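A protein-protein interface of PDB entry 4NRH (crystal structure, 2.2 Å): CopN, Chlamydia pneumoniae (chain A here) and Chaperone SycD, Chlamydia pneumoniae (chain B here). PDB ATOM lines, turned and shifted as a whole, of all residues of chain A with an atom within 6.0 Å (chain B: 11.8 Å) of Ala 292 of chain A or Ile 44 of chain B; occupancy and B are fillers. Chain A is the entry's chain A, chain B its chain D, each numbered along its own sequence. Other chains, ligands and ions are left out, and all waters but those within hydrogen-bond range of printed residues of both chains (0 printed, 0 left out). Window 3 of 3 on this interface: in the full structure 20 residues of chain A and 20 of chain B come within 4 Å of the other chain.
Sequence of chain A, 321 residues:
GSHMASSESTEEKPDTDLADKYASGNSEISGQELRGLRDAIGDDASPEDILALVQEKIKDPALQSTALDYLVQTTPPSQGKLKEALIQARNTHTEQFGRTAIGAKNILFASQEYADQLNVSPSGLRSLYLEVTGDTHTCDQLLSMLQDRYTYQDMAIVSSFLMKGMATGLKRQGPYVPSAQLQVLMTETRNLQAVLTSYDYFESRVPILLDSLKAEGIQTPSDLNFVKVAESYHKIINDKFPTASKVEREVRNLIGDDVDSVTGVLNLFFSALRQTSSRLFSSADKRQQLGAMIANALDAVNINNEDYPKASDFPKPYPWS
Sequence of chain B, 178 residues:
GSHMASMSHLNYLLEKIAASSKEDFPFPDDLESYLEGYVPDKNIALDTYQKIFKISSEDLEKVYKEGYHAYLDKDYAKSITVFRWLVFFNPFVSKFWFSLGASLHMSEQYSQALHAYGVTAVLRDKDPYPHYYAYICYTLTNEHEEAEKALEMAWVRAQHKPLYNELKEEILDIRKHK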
ATOM      1  N   PHE A 270      31.414 -14.993 -14.423  1.00  0.00           N
ATOM      2  CA  PHE A 270      30.075 -14.518 -14.094  1.00  0.00           C
ATOM      3  C   PHE A 270      29.134 -15.687 -13.825  1.00  0.00           C
ATOM      4  O   PHE A 270      28.337 -15.653 -12.888  1.00  0.00           O
ATOM      5  CB  PHE A 270      29.518 -13.640 -15.219  1.00  0.00           C
ATOM      6  CG  PHE A 270      28.254 -12.914 -14.851  1.00  0.00           C
ATOM      7  CD1 PHE A 270      27.016 -13.501 -15.054  1.00  0.00           C
ATOM      8  CD2 PHE A 270      28.305 -11.649 -14.289  1.00  0.00           C
ATOM      9  CE1 PHE A 270      25.853 -12.839 -14.709  1.00  0.00           C
ATOM     10  CE2 PHE A 270      27.147 -10.981 -13.942  1.00  0.00           C
ATOM     11  CZ  PHE A 270      25.919 -11.577 -14.153  1.00  0.00           C
ATOM     12  N   ARG A 287      29.538  -9.862  -3.517  1.00  0.00           N
ATOM     13  CA  ARG A 287      29.095 -10.785  -4.558  1.00  0.00           C
ATOM     14  C   ARG A 287      28.326 -10.028  -5.634  1.00  0.00           C
ATOM     15  O   ARG A 287      28.593 -10.181  -6.826  1.00  0.00           O
ATOM     16  CB  ARG A 287      28.221 -11.894  -3.970  1.00  0.00           C
ATOM     17  CG  ARG A 287      27.537 -12.743  -5.029  1.00  0.00           C
ATOM     18  CD  ARG A 287      26.819 -13.936  -4.425  1.00  0.00           C
ATOM     19  NE  ARG A 287      26.279 -14.810  -5.461  1.00  0.00           N
ATOM     20  CZ  ARG A 287      25.059 -14.694  -5.971  1.00  0.00           C
ATOM     21  NH1 ARG A 287      24.251 -13.734  -5.544  1.00  0.00           N
ATOM     22  NH2 ARG A 287      24.646 -15.534  -6.912  1.00  0.00           N
ATOM     23  N   GLN A 288      27.366  -9.218  -5.200  1.00  0.00           N
ATOM     24  CA  GLN A 288      26.588  -8.385  -6.109  1.00  0.00           C
ATOM     25  C   GLN A 288      27.480  -7.404  -6.868  1.00  0.00           C
ATOM     26  O   GLN A 288      27.356  -7.251  -8.084  1.00  0.00           O
ATOM     27  CB  GLN A 288      25.509  -7.621  -5.339  1.00  0.00           C
ATOM     28  CG  GLN A 288      24.764  -6.593  -6.170  1.00  0.00           C
ATOM     29  CD  GLN A 288      23.569  -6.012  -5.441  1.00  0.00           C
ATOM     30  OE1 GLN A 288      22.430  -6.423  -5.662  1.00  0.00           O
ATOM     31  NE2 GLN A 288      23.825  -5.051  -4.561  1.00  0.00           N
ATOM     32  N   GLN A 289      28.380  -6.747  -6.142  1.00  0.00           N
ATOM     33  CA  GLN A 289      29.296  -5.783  -6.743  1.00  0.00           C
ATOM     34  C   GLN A 289      30.253  -6.443  -7.731  1.00  0.00           C
ATOM     35  O   GLN A 289      30.602  -5.854  -8.753  1.00  0.00           O
ATOM     36  CB  GLN A 289      30.091  -5.050  -5.659  1.00  0.00           C
ATOM     37  CG  GLN A 289      30.942  -3.905  -6.188  1.00  0.00           C
ATOM     38  CD  GLN A 289      31.508  -3.036  -5.083  1.00  0.00           C
ATOM     39  OE1 GLN A 289      31.579  -3.451  -3.926  1.00  0.00           O
ATOM     40  NE2 GLN A 289      31.919  -1.824  -5.436  1.00  0.00           N
ATOM     41  N   LEU A 290      30.666  -7.671  -7.431  1.00  0.00           N
ATOM     42  CA  LEU A 290      31.572  -8.396  -8.315  1.00  0.00           C
ATOM     43  C   LEU A 290      30.865  -8.764  -9.615  1.00  0.00           C
ATOM     44  O   LEU A 290      31.456  -8.697 -10.692  1.00  0.00           O
ATOM     45  CB  LEU A 290      32.113  -9.653  -7.632  1.00  0.00           C
ATOM     46  CG  LEU A 290      33.105 -10.448  -8.480  1.00  0.00           C
ATOM     47  CD1 LEU A 290      34.199  -9.523  -8.979  1.00  0.00           C
ATOM     48  CD2 LEU A 290      33.697 -11.607  -7.690  1.00  0.00           C
ATOM     49  N   GLY A 291      29.599  -9.154  -9.501  1.00  0.00           N
ATOM     50  CA  GLY A 291      28.771  -9.428 -10.661  1.00  0.00           C
ATOM     51  C   GLY A 291      28.690  -8.214 -11.563  1.00  0.00           C
ATOM     52  O   GLY A 291      28.808  -8.323 -12.784  1.00  0.00           O
ATOM     53  N   ALA A 292      28.478  -7.054 -10.950  1.00  0.00           N
ATOM     54  CA  ALA A 292      28.422  -5.787 -11.670  1.00  0.00           C
ATOM     55  C   ALA A 292      29.724  -5.495 -12.410  1.00  0.00           C
ATOM     56  O   ALA A 292      29.710  -5.090 -13.572  1.00  0.00           O
ATOM     57  CB  ALA A 292      28.099  -4.653 -10.710  1.00  0.00           C
ATOM     58  N   MET A 293      30.848  -5.699 -11.730  1.00  0.00           N
ATOM     59  CA  MET A 293      32.154  -5.374 -12.295  1.00  0.00           C
ATOM     60  C   MET A 293      32.525  -6.299 -13.451  1.00  0.00           C
ATOM     61  O   MET A 293      33.150  -5.867 -14.420  1.00  0.00           O
ATOM     62  CB  MET A 293      33.234  -5.429 -11.212  1.00  0.00           C
ATOM     63  CG  MET A 293      33.078  -4.372 -10.128  1.00  0.00           C
ATOM     64  SD  MET A 293      32.883  -2.704 -10.788  1.00  0.00           S
ATOM     65  CE  MET A 293      31.162  -2.379 -10.406  1.00  0.00           C
ATOM     66  N   ILE A 294      32.144  -7.569 -13.349  1.00  0.00           N
ATOM     67  CA  ILE A 294      32.356  -8.513 -14.440  1.00  0.00           C
ATOM     68  C   ILE A 294      31.502  -8.113 -15.639  1.00  0.00           C
ATOM     69  O   ILE A 294      31.962  -8.145 -16.781  1.00  0.00           O
ATOM     70  CB  ILE A 294      32.028  -9.961 -14.021  1.00  0.00           C
ATOM     71  CG1 ILE A 294      32.997 -10.433 -12.936  1.00  0.00           C
ATOM     72  CG2 ILE A 294      32.100 -10.899 -15.218  1.00  0.00           C
ATOM     73  CD1 ILE A 294      32.641 -11.778 -12.345  1.00  0.00           C
ATOM     74  N   ALA A 295      30.258  -7.733 -15.365  1.00  0.00           N
ATOM     75  CA  ALA A 295      29.355  -7.234 -16.398  1.00  0.00           C
ATOM     76  C   ALA A 295      29.929  -5.987 -17.064  1.00  0.00           C
ATOM     77  O   ALA A 295      29.854  -5.830 -18.283  1.00  0.00           O
ATOM     78  CB  ALA A 295      27.984  -6.941 -15.809  1.00  0.00           C
ATOM     79  N   ASN A 296      30.502  -5.103 -16.252  1.00  0.00           N
ATOM     80  CA  ASN A 296      31.133  -3.891 -16.759  1.00  0.00           C
ATOM     81  C   ASN A 296      32.374  -4.207 -17.584  1.00  0.00           C
ATOM     82  O   ASN A 296      32.632  -3.567 -18.604  1.00  0.00           O
ATOM     83  CB  ASN A 296      31.501  -2.955 -15.605  1.00  0.00           C
ATOM     84  CG  ASN A 296      30.286  -2.317 -14.963  1.00  0.00           C
ATOM     85  OD1 ASN A 296      29.148  -2.596 -15.345  1.00  0.00           O
ATOM     86  ND2 ASN A 296      30.520  -1.450 -13.985  1.00  0.00           N
ATOM     87  N   ALA A 297      33.141  -5.195 -17.133  1.00  0.00           N
ATOM     88  CA  ALA A 297      34.349  -5.613 -17.835  1.00  0.00           C
ATOM     89  C   ALA A 297      34.018  -6.176 -19.211  1.00  0.00           C
ATOM     90  O   ALA A 297      34.714  -5.900 -20.187  1.00  0.00           O
ATOM     91  CB  ALA A 297      35.112  -6.641 -17.010  1.00  0.00           C
ATOM     92  N   TYR B  38      24.185  -4.318   3.002  1.00  0.00           N
ATOM     93  CA  TYR B  38      23.691  -4.849   1.738  1.00  0.00           C
ATOM     94  C   TYR B  38      22.442  -4.119   1.257  1.00  0.00           C
ATOM     95  O   TYR B  38      21.424  -4.085   1.948  1.00  0.00           O
ATOM     96  CB  TYR B  38      23.400  -6.343   1.878  1.00  0.00           C
ATOM     97  CG  TYR B  38      22.870  -7.005   0.626  1.00  0.00           C
ATOM     98  CD1 TYR B  38      23.466  -6.785  -0.610  1.00  0.00           C
ATOM     99  CD2 TYR B  38      21.783  -7.867   0.685  1.00  0.00           C
ATOM    100  CE1 TYR B  38      22.984  -7.398  -1.754  1.00  0.00           C
ATOM    101  CE2 TYR B  38      21.296  -8.483  -0.449  1.00  0.00           C
ATOM    102  CZ  TYR B  38      21.898  -8.247  -1.665  1.00  0.00           C
ATOM    103  OH  TYR B  38      21.410  -8.863  -2.794  1.00  0.00           O
ATOM    104  N   VAL B  39      22.529  -3.544   0.063  1.00  0.00           N
ATOM    105  CA  VAL B  39      21.368  -2.970  -0.605  1.00  0.00           C
ATOM    106  C   VAL B  39      21.176  -3.662  -1.947  1.00  0.00           C
ATOM    107  O   VAL B  39      21.931  -3.412  -2.888  1.00  0.00           O
ATOM    108  CB  VAL B  39      21.516  -1.450  -0.821  1.00  0.00           C
ATOM    109  CG1 VAL B  39      20.275  -0.885  -1.504  1.00  0.00           C
ATOM    110  CG2 VAL B  39      21.772  -0.747   0.502  1.00  0.00           C
ATOM    111  N   PRO B  40      20.167  -4.543  -2.035  1.00  0.00           N
ATOM    112  CA  PRO B  40      19.910  -5.331  -3.245  1.00  0.00           C
ATOM    113  C   PRO B  40      19.675  -4.451  -4.467  1.00  0.00           C
ATOM    114  O   PRO B  40      18.829  -3.556  -4.439  1.00  0.00           O
ATOM    115  CB  PRO B  40      18.647  -6.126  -2.891  1.00  0.00           C
ATOM    116  CG  PRO B  40      18.597  -6.133  -1.402  1.00  0.00           C
ATOM    117  CD  PRO B  40      19.206  -4.843  -0.961  1.00  0.00           C
ATOM    118  N   ASP B  41      20.422  -4.715  -5.532  1.00  0.00           N
ATOM    119  CA  ASP B  41      20.321  -3.928  -6.752  1.00  0.00           C
ATOM    120  C   ASP B  41      19.607  -4.748  -7.819  1.00  0.00           C
ATOM    121  O   ASP B  41      20.161  -5.705  -8.363  1.00  0.00           O
ATOM    122  CB  ASP B  41      21.710  -3.496  -7.230  1.00  0.00           C
ATOM    123  CG  ASP B  41      21.659  -2.419  -8.302  1.00  0.00           C
ATOM    124  OD1 ASP B  41      20.671  -2.359  -9.064  1.00  0.00           O
ATOM    125  OD2 ASP B  41      22.621  -1.627  -8.382  1.00  0.00           O
ATOM    126  N   LYS B  42      18.367  -4.364  -8.106  1.00  0.00           N
ATOM    127  CA  LYS B  42      17.514  -5.087  -9.044  1.00  0.00           C
ATOM    128  C   LYS B  42      18.043  -5.083 -10.478  1.00  0.00           C
ATOM    129  O   LYS B  42      17.559  -5.834 -11.323  1.00  0.00           O
ATOM    130  CB  LYS B  42      16.104  -4.493  -9.023  1.00  0.00           C
ATOM    131  CG  LYS B  42      16.058  -3.027  -9.421  1.00  0.00           C
ATOM    132  CD  LYS B  42      14.734  -2.384  -9.050  1.00  0.00           C
ATOM    133  CE  LYS B  42      14.699  -0.927  -9.478  1.00  0.00           C
ATOM    134  NZ  LYS B  42      13.402  -0.276  -9.145  1.00  0.00           N
ATOM    135  N   ASN B  43      19.035  -4.242 -10.749  1.00  0.00           N
ATOM    136  CA  ASN B  43      19.562  -4.108 -12.101  1.00  0.00           C
ATOM    137  C   ASN B  43      20.833  -4.921 -12.330  1.00  0.00           C
ATOM    138  O   ASN B  43      21.405  -4.900 -13.420  1.00  0.00           O
ATOM    139  CB  ASN B  43      19.825  -2.636 -12.420  1.00  0.00           C
ATOM    140  CG  ASN B  43      18.543  -1.839 -12.583  1.00  0.00           C
ATOM    141  OD1 ASN B  43      17.508  -2.377 -12.980  1.00  0.00           O
ATOM    142  ND2 ASN B  43      18.605  -0.548 -12.273  1.00  0.00           N
ATOM    143  N   ILE B  44      21.274  -5.634 -11.298  1.00  0.00           N
ATOM    144  CA  ILE B  44      22.373  -6.581 -11.449  1.00  0.00           C
ATOM    145  C   ILE B  44      21.817  -7.929 -11.890  1.00  0.00           C
ATOM    146  O   ILE B  44      21.003  -8.531 -11.191  1.00  0.00           O
ATOM    147  CB  ILE B  44      23.174  -6.749 -10.147  1.00  0.00           C
ATOM    148  CG1 ILE B  44      23.600  -5.383  -9.607  1.00  0.00           C
ATOM    149  CG2 ILE B  44      24.384  -7.640 -10.376  1.00  0.00           C
ATOM    150  CD1 ILE B  44      24.492  -4.608 -10.546  1.00  0.00           C
ATOM    151  N   ALA B  45      22.261  -8.400 -13.049  1.00  0.00           N
ATOM    152  CA  ALA B  45      21.695  -9.603 -13.648  1.00  0.00           C
ATOM    153  C   ALA B  45      22.220 -10.871 -12.978  1.00  0.00           C
ATOM    154  O   ALA B  45      22.857 -11.705 -13.620  1.00  0.00           O
ATOM    155  CB  ALA B  45      21.988  -9.634 -15.141  1.00  0.00           C
ATOM    156  N   LEU B  46      21.936 -11.011 -11.688  1.00  0.00           N
ATOM    157  CA  LEU B  46      22.354 -12.182 -10.925  1.00  0.00           C
ATOM    158  C   LEU B  46      21.148 -12.962 -10.416  1.00  0.00           C
ATOM    159  O   LEU B  46      20.192 -12.378  -9.904  1.00  0.00           O
ATOM    160  CB  LEU B  46      23.241 -11.768  -9.748  1.00  0.00           C
ATOM    161  CG  LEU B  46      24.752 -11.739  -9.975  1.00  0.00           C
ATOM    162  CD1 LEU B  46      25.467 -11.293  -8.709  1.00  0.00           C
ATOM    163  CD2 LEU B  46      25.258 -13.101 -10.427  1.00  0.00           C
ATOM    164  N   ASP B  47      21.195 -14.281 -10.564  1.00  0.00           N
ATOM    165  CA  ASP B  47      20.166 -15.147 -10.002  1.00  0.00           C
ATOM    166  C   ASP B  47      20.187 -15.106  -8.481  1.00  0.00           C
ATOM    167  O   ASP B  47      21.254 -15.104  -7.868  1.00  0.00           O
ATOM    168  CB  ASP B  47      20.345 -16.589 -10.487  1.00  0.00           C
ATOM    169  CG  ASP B  47      19.913 -16.778 -11.926  1.00  0.00           C
ATOM    170  OD1 ASP B  47      19.285 -15.854 -12.485  1.00  0.00           O
ATOM    171  OD2 ASP B  47      20.200 -17.850 -12.498  1.00  0.00           O
ATOM    172  N   THR B  48      19.006 -15.074  -7.876  1.00  0.00           N
ATOM    173  CA  THR B  48      18.896 -15.192  -6.429  1.00  0.00           C
ATOM    174  C   THR B  48      19.191 -16.630  -6.021  1.00  0.00           C
ATOM    175  O   THR B  48      19.164 -17.534  -6.856  1.00  0.00           O
ATOM    176  CB  THR B  48      17.499 -14.791  -5.926  1.00  0.00           C
ATOM    177  OG1 THR B  48      16.525 -15.703  -6.447  1.00  0.00           O
ATOM    178  CG2 THR B  48      17.153 -13.373  -6.365  1.00  0.00           C
ATOM    179  N   TYR B  49      19.471 -16.845  -4.741  1.00  0.00           N
ATOM    180  CA  TYR B  49      19.738 -18.194  -4.252  1.00  0.00           C
ATOM    181  C   TYR B  49      18.462 -19.029  -4.196  1.00  0.00           C
ATOM    182  O   TYR B  49      18.521 -20.257  -4.211  1.00  0.00           O
ATOM    183  CB  TYR B  49      20.430 -18.146  -2.890  1.00  0.00           C
ATOM    184  CG  TYR B  49      21.905 -17.833  -3.019  1.00  0.00           C
ATOM    185  CD1 TYR B  49      22.759 -18.706  -3.679  1.00  0.00           C
ATOM    186  CD2 TYR B  49      22.439 -16.660  -2.503  1.00  0.00           C
ATOM    187  CE1 TYR B  49      24.104 -18.427  -3.815  1.00  0.00           C
ATOM    188  CE2 TYR B  49      23.786 -16.372  -2.632  1.00  0.00           C
ATOM    189  CZ  TYR B  49      24.614 -17.260  -3.291  1.00  0.00           C
ATOM    190  OH  TYR B  49      25.954 -16.983  -3.422  1.00  0.00           O
ATOM    191  N   LYS B  51      16.386 -18.959  -6.656  1.00  0.00           N
ATOM    192  CA  LYS B  51      16.444 -19.448  -8.027  1.00  0.00           C
ATOM    193  C   LYS B  51      17.459 -20.578  -8.167  1.00  0.00           C
ATOM    194  O   LYS B  51      17.149 -21.643  -8.701  1.00  0.00           O
ATOM    195  CB  LYS B  51      16.796 -18.303  -8.979  1.00  0.00           C
ATOM    196  CG  LYS B  51      17.120 -18.736 -10.396  1.00  0.00           C
ATOM    197  CD  LYS B  51      15.879 -19.216 -11.124  1.00  0.00           C
ATOM    198  CE  LYS B  51      16.133 -19.332 -12.618  1.00  0.00           C
ATOM    199  NZ  LYS B  51      14.903 -19.715 -13.364  1.00  0.00           N
ATOM    200  N   ILE B  52      18.674 -20.325  -7.687  1.00  0.00           N
ATOM    201  CA  ILE B  52      19.767 -21.291  -7.754  1.00  0.00           C
ATOM    202  C   ILE B  52      19.432 -22.616  -7.066  1.00  0.00           C
ATOM    203  O   ILE B  52      19.724 -23.689  -7.596  1.00  0.00           O
ATOM    204  CB  ILE B  52      21.052 -20.706  -7.129  1.00  0.00           C
ATOM    205  CG1 ILE B  52      21.533 -19.501  -7.942  1.00  0.00           C
ATOM    206  CG2 ILE B  52      22.145 -21.762  -7.039  1.00  0.00           C
ATOM    207  CD1 ILE B  52      22.559 -18.650  -7.227  1.00  0.00           C
ATOM    208  N   ASN B  90      15.956 -14.635  -1.138  1.00  0.00           N
ATOM    209  CA  ASN B  90      15.388 -13.660  -2.060  1.00  0.00           C
ATOM    210  C   ASN B  90      15.307 -12.283  -1.407  1.00  0.00           C
ATOM    211  O   ASN B  90      14.317 -11.962  -0.750  1.00  0.00           O
ATOM    212  CB  ASN B  90      14.001 -14.110  -2.533  1.00  0.00           C
ATOM    213  CG  ASN B  90      13.485 -13.298  -3.714  1.00  0.00           C
ATOM    214  OD1 ASN B  90      13.935 -12.181  -3.968  1.00  0.00           O
ATOM    215  ND2 ASN B  90      12.525 -13.863  -4.439  1.00  0.00           N
ATOM    216  N   PRO B  91      16.352 -11.464  -1.594  1.00  0.00           N
ATOM    217  CA  PRO B  91      16.456 -10.138  -0.974  1.00  0.00           C
ATOM    218  C   PRO B  91      15.621  -9.067  -1.672  1.00  0.00           C
ATOM    219  O   PRO B  91      15.698  -7.899  -1.292  1.00  0.00           O
ATOM    220  CB  PRO B  91      17.945  -9.816  -1.101  1.00  0.00           C
ATOM    221  CG  PRO B  91      18.364 -10.527  -2.338  1.00  0.00           C
ATOM    222  CD  PRO B  91      17.547 -11.793  -2.392  1.00  0.00           C
ATOM    223  N   PHE B  92      14.838  -9.456  -2.673  1.00  0.00           N
ATOM    224  CA  PHE B  92      14.024  -8.494  -3.411  1.00  0.00           C
ATOM    225  C   PHE B  92      12.564  -8.517  -2.972  1.00  0.00           C
ATOM    226  O   PHE B  92      11.728  -7.813  -3.537  1.00  0.00           O
ATOM    227  CB  PHE B  92      14.130  -8.751  -4.916  1.00  0.00           C
ATOM    228  CG  PHE B  92      15.529  -8.635  -5.449  1.00  0.00           C
ATOM    229  CD1 PHE B  92      16.087  -7.392  -5.697  1.00  0.00           C
ATOM    230  CD2 PHE B  92      16.287  -9.767  -5.700  1.00  0.00           C
ATOM    231  CE1 PHE B  92      17.374  -7.279  -6.184  1.00  0.00           C
ATOM    232  CE2 PHE B  92      17.576  -9.660  -6.188  1.00  0.00           C
ATOM    233  CZ  PHE B  92      18.119  -8.414  -6.430  1.00  0.00           C
ATOM    234  N   VAL B 122      13.736   1.234  -0.508  1.00  0.00           N
ATOM    235  CA  VAL B 122      14.278   1.099  -1.857  1.00  0.00           C
ATOM    236  C   VAL B 122      13.434   0.148  -2.704  1.00  0.00           C
ATOM    237  O   VAL B 122      13.117   0.439  -3.859  1.00  0.00           O
ATOM    238  CB  VAL B 122      15.735   0.592  -1.824  1.00  0.00           C
ATOM    239  CG1 VAL B 122      16.238   0.310  -3.232  1.00  0.00           C
ATOM    240  CG2 VAL B 122      16.631   1.603  -1.127  1.00  0.00           C
ATOM    241  N   LEU B 123      13.068  -0.987  -2.118  1.00  0.00           N
ATOM    242  CA  LEU B 123      12.302  -2.010  -2.822  1.00  0.00           C
ATOM    243  C   LEU B 123      10.839  -1.607  -2.993  1.00  0.00           C
ATOM    244  O   LEU B 123      10.138  -2.130  -3.859  1.00  0.00           O
ATOM    245  CB  LEU B 123      12.393  -3.343  -2.077  1.00  0.00           C
ATOM    246  CG  LEU B 123      13.791  -3.949  -1.926  1.00  0.00           C
ATOM    247  CD1 LEU B 123      13.742  -5.200  -1.059  1.00  0.00           C
ATOM    248  CD2 LEU B 123      14.406  -4.256  -3.285  1.00  0.00           C
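Printed residues of chain B that touch a printed residue of chain A: Tyr 38, Val 39, Pro 40, Asp 41, Ile 44, Ala 45, Leu 46, Asp 47, Tyr 49 and Ile 52.
Of the 12 printed residues of chain A, 4 touch a printed residue of chain B.
Hydrophobic or aromatic side chains of chain A within 4 Å of the printed part of chain B: Phe 270 and Ala 292.
Along chain A the printed residues that touch a printed residue of chain B span positions 270 to 292.
Among the printed residues, 11 pairs touch across the chains.
Among the printed residues, no Asp or Glu carboxylate lies within 4 Å of a Lys or Arg side-chain nitrogen of the other chain.
Ala 45 of chain B touches Phe 270 of chain A.
Arg 287 of chain A touches Leu 46 of chain B (O to CD1, 3.8 Å).
Asp 47 of chain B touches Arg 287 of chain A.
Arg 287 of chain A touches Ile 52 of chain B.
Gln 288 of chain A touches Tyr 38 of chain B (NE2 to CE1, 3.8 Å).
OE1 of Gln 288 of chain A touches C of Pro 40 of chain B, 3.6 Å away.
O of Gln 288 of chain A touches CG2 of Ile 44 of chain B, at 3.8 Å.
CB of Ala 292 of chain A touches CD1 of Ile 44 of chain B (3.6 Å).
Ala 292 of chain A touches just one residue of chain B: Ile 44 (3.6 Å).
Gln 288 of chain A touches just these residues of chain B: Tyr 38 (3.8 Å), Val 39 (3.0 Å), Pro 40 (3.6 Å), Asp 41 (2.6 Å) and Ile 44 (3.8 Å).
No residue of chain B comes within 4 Å of Gln 289 of chain A.
No residue of chain B comes within 4 Å of Leu 290 of chain A.
No residue of chain B comes within 4 Å of Gly 291 of chain A.
No residue of chain B comes within 4 Å of Ala 295 of chain A.
Printed residues of chain B within 4 Å of Phe 270 of chain A: Ala 45.
Printed residues of chain A within 4 Å of Asp 41 of chain B: Gln 288.
Ala 297 of chain A touches none of the printed residues of chain B.
O of Ala 292 of chain A sits close to OD1 of Asn 296 of chain A, at 3.1 Å.
The side-chain carboxylate of Asp 41 of chain B lies within hydrogen-bond range of the backbone NH of Asn 43 of chain B (3.0 Å).
The side-chain hydroxyl of Tyr 49 of chain B is in hydrogen-bond range of the guanidinium group of Arg 287 of chain A, at 3.0 Å.
The side-chain amide nitrogen of Gln 288 of chain A sits at hydrogen-bond distance from the backbone carbonyl oxygen of Val 39 of chain B (3.0 Å).
N of Asp 41 of chain B lies within hydrogen-bond range of OE1 of Gln 288 of chain A (2.6 Å).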
